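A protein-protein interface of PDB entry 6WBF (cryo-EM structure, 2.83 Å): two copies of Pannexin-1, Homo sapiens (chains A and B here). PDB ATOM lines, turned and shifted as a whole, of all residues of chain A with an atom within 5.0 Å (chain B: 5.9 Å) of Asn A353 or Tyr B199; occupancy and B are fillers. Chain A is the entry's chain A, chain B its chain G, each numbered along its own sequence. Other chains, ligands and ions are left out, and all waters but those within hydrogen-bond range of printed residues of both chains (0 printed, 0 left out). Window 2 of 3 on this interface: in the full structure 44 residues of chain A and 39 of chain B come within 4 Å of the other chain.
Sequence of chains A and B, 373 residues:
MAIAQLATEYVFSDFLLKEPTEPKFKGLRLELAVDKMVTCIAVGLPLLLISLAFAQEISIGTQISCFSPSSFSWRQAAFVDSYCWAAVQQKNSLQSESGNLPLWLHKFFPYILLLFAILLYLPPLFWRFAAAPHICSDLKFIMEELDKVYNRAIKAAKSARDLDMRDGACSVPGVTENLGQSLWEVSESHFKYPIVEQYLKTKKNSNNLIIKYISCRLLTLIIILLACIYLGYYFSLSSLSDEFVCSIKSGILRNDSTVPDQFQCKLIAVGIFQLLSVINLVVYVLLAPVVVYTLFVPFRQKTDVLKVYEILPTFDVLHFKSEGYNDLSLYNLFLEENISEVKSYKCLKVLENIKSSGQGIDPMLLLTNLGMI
Printed residues of chain A that touch a printed residue of chain B: Lys A346, Val A350, Asn A353 and Ile A354.
Hydrophobic or aromatic side chains of chain A that line the printed part of chain B: Val A350 and Ile A354.
Among the printed residues, 8 pairs touch across the chains.
Among the printed residues, pairs that only touch across the chains: Lys A346 with Phe B141 (3.9 Å), Val A350 with Phe B141 (3.5 Å), Asn A353 with Tyr B199 (3.9 Å), Ile A354 with Ile B195 (3.8 Å) and Ile A354 with Thr B202 (3.8 Å).
The side-chain carboxylate (OE1) of Glu A352 sits close to the side-chain amide oxygen (OD1) of Asn A353 (3.3 Å).
The side-chain carboxylate of Asp B138 sits close to the side-chain hydroxyl of Tyr B199 (3.4 Å).
NZ of Lys B203 lies within salt-bridge range of OD2 of Asp B138 (3.8 Å).
The backbone carbonyl oxygen (O) of Gln B198 sits at hydrogen-bond distance from the side-chain hydroxyl (OG1) of Thr B202 (3.0 Å).
NZ of Lys A346 lies within salt-bridge range of OD1 of Asp B138, 3.0 Å away.
The side-chain hydroxyl of Tyr B199 is in hydrogen-bond range of the side-chain amino group of Lys A346, 3.5 Å away.
The backbone carbonyl oxygen of Asn A353 sits at hydrogen-bond distance from the side-chain hydroxyl of Thr B202, at 3.4 Å.
No position is printed for both chains.
Of the 8 pairs that touch across the chains among the printed residues, none has its exchanged pair printed and touching as well.
Asn A353 touches just these residues of chain B: Tyr B199 and Thr B202.
Of chain A, only Lys A346 and Asn A353 come within 4 Å of Tyr B199.
Of the printed residues of chain A, Thr B202 touches Asn A353 and Ile A354.
Printed residues of chain B within 4 Å of Lys A346: Asp B138, Phe B141 and Tyr B199.
Of the printed residues of chain B, Val A350 touches Phe B141 (3.5 Å).
Of the printed residues of chain A, Ile B195 touches Ile A354 (3.8 Å).
Of the printed residues of chain A, Asp B138 touches Lys A346.
Lys B201 touches none of the printed residues of chain A.
The nearest residue of chain A that does not touch Tyr B199 is Val A350 (4.1 Å).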
ATOM      1  N   LYS A 346      20.426   9.833 -27.531  1.00  0.00           N
ATOM      2  CA  LYS A 346      19.060  10.251 -27.242  1.00  0.00           C
ATOM      3  C   LYS A 346      18.965  10.897 -25.868  1.00  0.00           C
ATOM      4  O   LYS A 346      18.400  11.987 -25.723  1.00  0.00           O
ATOM      5  CB  LYS A 346      18.113   9.060 -27.343  1.00  0.00           C
ATOM      6  CG  LYS A 346      16.663   9.441 -27.151  1.00  0.00           C
ATOM      7  CD  LYS A 346      16.253  10.469 -28.188  1.00  0.00           C
ATOM      8  CE  LYS A 346      14.820  10.916 -27.990  1.00  0.00           C
ATOM      9  NZ  LYS A 346      14.661  11.762 -26.785  1.00  0.00           N
ATOM     10  N   LYS A 349      20.693  14.255 -25.793  1.00  0.00           N
ATOM     11  CA  LYS A 349      19.918  15.295 -26.456  1.00  0.00           C
ATOM     12  C   LYS A 349      18.739  15.723 -25.598  1.00  0.00           C
ATOM     13  O   LYS A 349      18.356  16.898 -25.598  1.00  0.00           O
ATOM     14  CB  LYS A 349      19.450  14.816 -27.829  1.00  0.00           C
ATOM     15  CG  LYS A 349      18.507  15.782 -28.523  1.00  0.00           C
ATOM     16  CD  LYS A 349      18.755  15.819 -30.018  1.00  0.00           C
ATOM     17  CE  LYS A 349      19.880  16.785 -30.353  1.00  0.00           C
ATOM     18  NZ  LYS A 349      19.517  18.193 -30.042  1.00  0.00           N
ATOM     19  N   VAL A 350      18.152  14.783 -24.854  1.00  0.00           N
ATOM     20  CA  VAL A 350      17.155  15.166 -23.862  1.00  0.00           C
ATOM     21  C   VAL A 350      17.723  16.168 -22.877  1.00  0.00           C
ATOM     22  O   VAL A 350      17.110  17.213 -22.631  1.00  0.00           O
ATOM     23  CB  VAL A 350      16.608  13.945 -23.106  1.00  0.00           C
ATOM     24  CG1 VAL A 350      15.594  14.398 -22.083  1.00  0.00           C
ATOM     25  CG2 VAL A 350      15.969  12.974 -24.063  1.00  0.00           C
ATOM     26  N   LEU A 351      18.890  15.879 -22.302  1.00  0.00           N
ATOM     27  CA  LEU A 351      19.497  16.831 -21.376  1.00  0.00           C
ATOM     28  C   LEU A 351      19.830  18.156 -22.054  1.00  0.00           C
ATOM     29  O   LEU A 351      19.660  19.222 -21.455  1.00  0.00           O
ATOM     30  CB  LEU A 351      20.749  16.239 -20.730  1.00  0.00           C
ATOM     31  CG  LEU A 351      20.572  15.317 -19.518  1.00  0.00           C
ATOM     32  CD1 LEU A 351      20.004  13.962 -19.876  1.00  0.00           C
ATOM     33  CD2 LEU A 351      21.905  15.164 -18.811  1.00  0.00           C
ATOM     34  N   GLU A 352      20.294  18.110 -23.302  1.00  0.00           N
ATOM     35  CA  GLU A 352      20.671  19.337 -23.993  1.00  0.00           C
ATOM     36  C   GLU A 352      19.458  20.217 -24.251  1.00  0.00           C
ATOM     37  O   GLU A 352      19.534  21.445 -24.131  1.00  0.00           O
ATOM     38  CB  GLU A 352      21.384  18.996 -25.301  1.00  0.00           C
ATOM     39  CG  GLU A 352      22.205  20.133 -25.877  1.00  0.00           C
ATOM     40  CD  GLU A 352      21.399  21.015 -26.809  1.00  0.00           C
ATOM     41  OE1 GLU A 352      20.436  20.507 -27.418  1.00  0.00           O
ATOM     42  OE2 GLU A 352      21.731  22.212 -26.933  1.00  0.00           O
ATOM     43  N   ASN A 353      18.327  19.609 -24.611  1.00  0.00           N
ATOM     44  CA  ASN A 353      17.106  20.376 -24.833  1.00  0.00           C
ATOM     45  C   ASN A 353      16.599  20.979 -23.533  1.00  0.00           C
ATOM     46  O   ASN A 353      16.128  22.121 -23.504  1.00  0.00           O
ATOM     47  CB  ASN A 353      16.039  19.486 -25.469  1.00  0.00           C
ATOM     48  CG  ASN A 353      16.265  19.275 -26.949  1.00  0.00           C
ATOM     49  OD1 ASN A 353      17.224  19.794 -27.520  1.00  0.00           O
ATOM     50  ND2 ASN A 353      15.383  18.510 -27.580  1.00  0.00           N
ATOM     51  N   ILE A 354      16.678  20.218 -22.441  1.00  0.00           N
ATOM     52  CA  ILE A 354      16.301  20.750 -21.137  1.00  0.00           C
ATOM     53  C   ILE A 354      17.193  21.927 -20.770  1.00  0.00           C
ATOM     54  O   ILE A 354      16.740  22.910 -20.169  1.00  0.00           O
ATOM     55  CB  ILE A 354      16.359  19.639 -20.072  1.00  0.00           C
ATOM     56  CG1 ILE A 354      15.301  18.576 -20.360  1.00  0.00           C
ATOM     57  CG2 ILE A 354      16.160  20.212 -18.685  1.00  0.00           C
ATOM     58  CD1 ILE A 354      15.435  17.347 -19.499  1.00  0.00           C
ATOM     59  N   LYS A 355      18.471  21.856 -21.143  1.00  0.00           N
ATOM     60  CA  LYS A 355      19.422  22.917 -20.842  1.00  0.00           C
ATOM     61  C   LYS A 355      19.039  24.241 -21.492  1.00  0.00           C
ATOM     62  O   LYS A 355      19.559  25.292 -21.110  1.00  0.00           O
ATOM     63  CB  LYS A 355      20.830  22.509 -21.278  1.00  0.00           C
ATOM     64  CG  LYS A 355      21.588  21.701 -20.243  1.00  0.00           C
ATOM     65  CD  LYS A 355      21.619  22.418 -18.905  1.00  0.00           C
ATOM     66  CE  LYS A 355      22.441  23.695 -18.981  1.00  0.00           C
ATOM     67  NZ  LYS A 355      23.829  23.436 -19.451  1.00  0.00           N
ATOM     68  N   SER A 356      18.149  24.201 -22.485  1.00  0.00           N
ATOM     69  CA  SER A 356      17.665  25.438 -23.090  1.00  0.00           C
ATOM     70  C   SER A 356      16.975  26.315 -22.055  1.00  0.00           C
ATOM     71  O   SER A 356      17.140  27.540 -22.047  1.00  0.00           O
ATOM     72  CB  SER A 356      16.723  25.129 -24.251  1.00  0.00           C
ATOM     73  N   SER A 357      16.192  25.700 -21.166  1.00  0.00           N
ATOM     74  CA  SER A 357      15.602  26.448 -20.060  1.00  0.00           C
ATOM     75  C   SER A 357      16.664  26.823 -19.035  1.00  0.00           C
ATOM     76  O   SER A 357      16.616  27.910 -18.444  1.00  0.00           O
ATOM     77  CB  SER A 357      14.486  25.632 -19.411  1.00  0.00           C
ATOM     78  N   ASP B 138      11.407  10.282 -29.313  1.00  0.00           N
ATOM     79  CA  ASP B 138      10.936  11.076 -28.184  1.00  0.00           C
ATOM     80  C   ASP B 138       9.806  10.378 -27.442  1.00  0.00           C
ATOM     81  O   ASP B 138       9.776  10.384 -26.208  1.00  0.00           O
ATOM     82  CB  ASP B 138      10.476  12.449 -28.666  1.00  0.00           C
ATOM     83  CG  ASP B 138      11.618  13.313 -29.135  1.00  0.00           C
ATOM     84  OD1 ASP B 138      12.739  13.143 -28.620  1.00  0.00           O
ATOM     85  OD2 ASP B 138      11.394  14.168 -30.018  1.00  0.00           O
ATOM     86  N   PHE B 141      11.119   7.460 -25.447  1.00  0.00           N
ATOM     87  CA  PHE B 141      11.804   7.954 -24.260  1.00  0.00           C
ATOM     88  C   PHE B 141      10.812   8.422 -23.204  1.00  0.00           C
ATOM     89  O   PHE B 141      11.013   8.177 -22.011  1.00  0.00           O
ATOM     90  CB  PHE B 141      12.753   9.088 -24.633  1.00  0.00           C
ATOM     91  CG  PHE B 141      13.231   9.879 -23.455  1.00  0.00           C
ATOM     92  CD1 PHE B 141      14.245   9.398 -22.652  1.00  0.00           C
ATOM     93  CD2 PHE B 141      12.658  11.098 -23.143  1.00  0.00           C
ATOM     94  CE1 PHE B 141      14.685  10.118 -21.564  1.00  0.00           C
ATOM     95  CE2 PHE B 141      13.091  11.822 -22.055  1.00  0.00           C
ATOM     96  CZ  PHE B 141      14.106  11.331 -21.265  1.00  0.00           C
ATOM     97  N   ILE B 142       9.744   9.103 -23.620  1.00  0.00           N
ATOM     98  CA  ILE B 142       8.756   9.586 -22.662  1.00  0.00           C
ATOM     99  C   ILE B 142       8.054   8.416 -21.987  1.00  0.00           C
ATOM    100  O   ILE B 142       7.817   8.431 -20.775  1.00  0.00           O
ATOM    101  CB  ILE B 142       7.755  10.527 -23.348  1.00  0.00           C
ATOM    102  CG1 ILE B 142       8.429  11.850 -23.703  1.00  0.00           C
ATOM    103  CG2 ILE B 142       6.560  10.778 -22.454  1.00  0.00           C
ATOM    104  CD1 ILE B 142       7.664  12.665 -24.714  1.00  0.00           C
ATOM    105  N   PRO B 194      11.915  16.182 -12.180  1.00  0.00           N
ATOM    106  CA  PRO B 194      10.902  15.909 -13.204  1.00  0.00           C
ATOM    107  C   PRO B 194      11.483  16.034 -14.602  1.00  0.00           C
ATOM    108  O   PRO B 194      11.298  17.053 -15.274  1.00  0.00           O
ATOM    109  CB  PRO B 194       9.835  16.974 -12.936  1.00  0.00           C
ATOM    110  CG  PRO B 194      10.588  18.102 -12.319  1.00  0.00           C
ATOM    111  CD  PRO B 194      11.712  17.486 -11.528  1.00  0.00           C
ATOM    112  N   ILE B 195      12.193  14.997 -15.049  1.00  0.00           N
ATOM    113  CA  ILE B 195      12.900  15.081 -16.321  1.00  0.00           C
ATOM    114  C   ILE B 195      11.920  15.067 -17.488  1.00  0.00           C
ATOM    115  O   ILE B 195      12.077  15.822 -18.452  1.00  0.00           O
ATOM    116  CB  ILE B 195      13.942  13.955 -16.431  1.00  0.00           C
ATOM    117  CG1 ILE B 195      14.658  14.018 -17.780  1.00  0.00           C
ATOM    118  CG2 ILE B 195      13.304  12.591 -16.208  1.00  0.00           C
ATOM    119  CD1 ILE B 195      15.882  13.140 -17.857  1.00  0.00           C
ATOM    120  N   VAL B 196      10.889  14.222 -17.421  1.00  0.00           N
ATOM    121  CA  VAL B 196       9.939  14.141 -18.524  1.00  0.00           C
ATOM    122  C   VAL B 196       9.089  15.404 -18.582  1.00  0.00           C
ATOM    123  O   VAL B 196       8.743  15.891 -19.667  1.00  0.00           O
ATOM    124  CB  VAL B 196       9.083  12.866 -18.406  1.00  0.00           C
ATOM    125  CG1 VAL B 196       8.170  12.926 -17.194  1.00  0.00           C
ATOM    126  CG2 VAL B 196       8.278  12.655 -19.672  1.00  0.00           C
ATOM    127  N   GLU B 197       8.768  15.977 -17.421  1.00  0.00           N
ATOM    128  CA  GLU B 197       8.026  17.230 -17.405  1.00  0.00           C
ATOM    129  C   GLU B 197       8.845  18.353 -18.024  1.00  0.00           C
ATOM    130  O   GLU B 197       8.318  19.168 -18.790  1.00  0.00           O
ATOM    131  CB  GLU B 197       7.619  17.575 -15.974  1.00  0.00           C
ATOM    132  CG  GLU B 197       6.583  18.678 -15.867  1.00  0.00           C
ATOM    133  CD  GLU B 197       7.204  20.048 -15.698  1.00  0.00           C
ATOM    134  OE1 GLU B 197       8.326  20.126 -15.158  1.00  0.00           O
ATOM    135  OE2 GLU B 197       6.571  21.046 -16.100  1.00  0.00           O
ATOM    136  N   GLN B 198      10.144  18.401 -17.722  1.00  0.00           N
ATOM    137  CA  GLN B 198      11.000  19.415 -18.326  1.00  0.00           C
ATOM    138  C   GLN B 198      11.150  19.187 -19.824  1.00  0.00           C
ATOM    139  O   GLN B 198      11.191  20.146 -20.604  1.00  0.00           O
ATOM    140  CB  GLN B 198      12.365  19.423 -17.643  1.00  0.00           C
ATOM    141  CG  GLN B 198      12.398  20.203 -16.343  1.00  0.00           C
ATOM    142  CD  GLN B 198      12.010  21.656 -16.526  1.00  0.00           C
ATOM    143  OE1 GLN B 198      11.175  22.185 -15.794  1.00  0.00           O
ATOM    144  NE2 GLN B 198      12.617  22.311 -17.510  1.00  0.00           N
ATOM    145  N   TYR B 199      11.218  17.925 -20.247  1.00  0.00           N
ATOM    146  CA  TYR B 199      11.311  17.627 -21.671  1.00  0.00           C
ATOM    147  C   TYR B 199      10.070  18.107 -22.412  1.00  0.00           C
ATOM    148  O   TYR B 199      10.164  18.690 -23.498  1.00  0.00           O
ATOM    149  CB  TYR B 199      11.511  16.129 -21.881  1.00  0.00           C
ATOM    150  CG  TYR B 199      11.945  15.782 -23.278  1.00  0.00           C
ATOM    151  CD1 TYR B 199      12.716  16.662 -24.017  1.00  0.00           C
ATOM    152  CD2 TYR B 199      11.580  14.580 -23.864  1.00  0.00           C
ATOM    153  CE1 TYR B 199      13.120  16.358 -25.295  1.00  0.00           C
ATOM    154  CE2 TYR B 199      11.978  14.266 -25.145  1.00  0.00           C
ATOM    155  CZ  TYR B 199      12.748  15.160 -25.854  1.00  0.00           C
ATOM    156  OH  TYR B 199      13.151  14.858 -27.132  1.00  0.00           O
ATOM    157  N   LEU B 200       8.893  17.868 -21.838  1.00  0.00           N
ATOM    158  CA  LEU B 200       7.665  18.330 -22.472  1.00  0.00           C
ATOM    159  C   LEU B 200       7.570  19.850 -22.449  1.00  0.00           C
ATOM    160  O   LEU B 200       7.093  20.467 -23.410  1.00  0.00           O
ATOM    161  CB  LEU B 200       6.462  17.693 -21.787  1.00  0.00           C
ATOM    162  CG  LEU B 200       6.484  16.171 -21.913  1.00  0.00           C
ATOM    163  CD1 LEU B 200       5.509  15.535 -20.949  1.00  0.00           C
ATOM    164  CD2 LEU B 200       6.182  15.752 -23.339  1.00  0.00           C
ATOM    165  N   LYS B 201       8.019  20.473 -21.359  1.00  0.00           N
ATOM    166  CA  LYS B 201       8.102  21.928 -21.325  1.00  0.00           C
ATOM    167  C   LYS B 201       8.976  22.448 -22.459  1.00  0.00           C
ATOM    168  O   LYS B 201       8.682  23.494 -23.051  1.00  0.00           O
ATOM    169  CB  LYS B 201       8.654  22.384 -19.976  1.00  0.00           C
ATOM    170  CG  LYS B 201       8.648  23.884 -19.776  1.00  0.00           C
ATOM    171  CD  LYS B 201       7.234  24.395 -19.598  1.00  0.00           C
ATOM    172  CE  LYS B 201       6.586  23.770 -18.377  1.00  0.00           C
ATOM    173  NZ  LYS B 201       7.310  24.135 -17.131  1.00  0.00           N
ATOM    174  N   THR B 202      10.055  21.732 -22.768  1.00  0.00           N
ATOM    175  CA  THR B 202      10.901  22.126 -23.890  1.00  0.00           C
ATOM    176  C   THR B 202      10.173  21.939 -25.214  1.00  0.00           C
ATOM    177  O   THR B 202      10.234  22.810 -26.092  1.00  0.00           O
ATOM    178  CB  THR B 202      12.197  21.320 -23.876  1.00  0.00           C
ATOM    179  OG1 THR B 202      12.900  21.577 -22.655  1.00  0.00           O
ATOM    180  CG2 THR B 202      13.076  21.722 -25.051  1.00  0.00           C
ATOM    181  N   LYS B 203       9.486  20.808 -25.378  1.00  0.00           N
ATOM    182  CA  LYS B 203       8.702  20.574 -26.588  1.00  0.00           C
ATOM    183  C   LYS B 203       7.679  21.678 -26.807  1.00  0.00           C
ATOM    184  O   LYS B 203       7.335  21.998 -27.949  1.00  0.00           O
ATOM    185  CB  LYS B 203       8.007  19.214 -26.516  1.00  0.00           C
ATOM    186  CG  LYS B 203       8.930  18.008 -26.443  1.00  0.00           C
ATOM    187  CD  LYS B 203       9.571  17.689 -27.783  1.00  0.00           C
ATOM    188  CE  LYS B 203      10.960  18.282 -27.911  1.00  0.00           C
ATOM    189  NZ  LYS B 203      11.616  17.867 -29.178  1.00  0.00           N
ATOM    190  N   LYS B 204       7.185  22.272 -25.722  1.00  0.00           N
ATOM    191  CA  LYS B 204       6.216  23.361 -25.810  1.00  0.00           C
ATOM    192  C   LYS B 204       6.763  24.549 -26.594  1.00  0.00           C
ATOM    193  O   LYS B 204       5.998  25.398 -27.058  1.00  0.00           O
ATOM    194  CB  LYS B 204       5.796  23.814 -24.410  1.00  0.00           C
ATOM    195  CG  LYS B 204       4.607  24.768 -24.384  1.00  0.00           C
ATOM    196  CD  LYS B 204       4.392  25.352 -22.998  1.00  0.00           C
ATOM    197  CE  LYS B 204       3.860  24.307 -22.032  1.00  0.00           C
ATOM    198  NZ  LYS B 204       3.517  24.887 -20.705  1.00  0.00           N
ATOM    199  N   TYR B 331       2.684  16.105 -29.670  1.00  0.00           N
ATOM    200  CA  TYR B 331       3.134  15.057 -28.765  1.00  0.00           C
ATOM    201  C   TYR B 331       2.012  14.618 -27.841  1.00  0.00           C
ATOM    202  O   TYR B 331       1.937  13.448 -27.466  1.00  0.00           O
ATOM    203  CB  TYR B 331       4.338  15.539 -27.963  1.00  0.00           C
ATOM    204  CG  TYR B 331       5.641  15.307 -28.677  1.00  0.00           C
ATOM    205  CD1 TYR B 331       6.259  14.071 -28.639  1.00  0.00           C
ATOM    206  CD2 TYR B 331       6.247  16.321 -29.399  1.00  0.00           C
ATOM    207  CE1 TYR B 331       7.446  13.856 -29.294  1.00  0.00           C
ATOM    208  CE2 TYR B 331       7.432  16.114 -30.058  1.00  0.00           C
ATOM    209  CZ  TYR B 331       8.029  14.881 -30.004  1.00  0.00           C
ATOM    210  OH  TYR B 331       9.216  14.675 -30.662  1.00  0.00           O
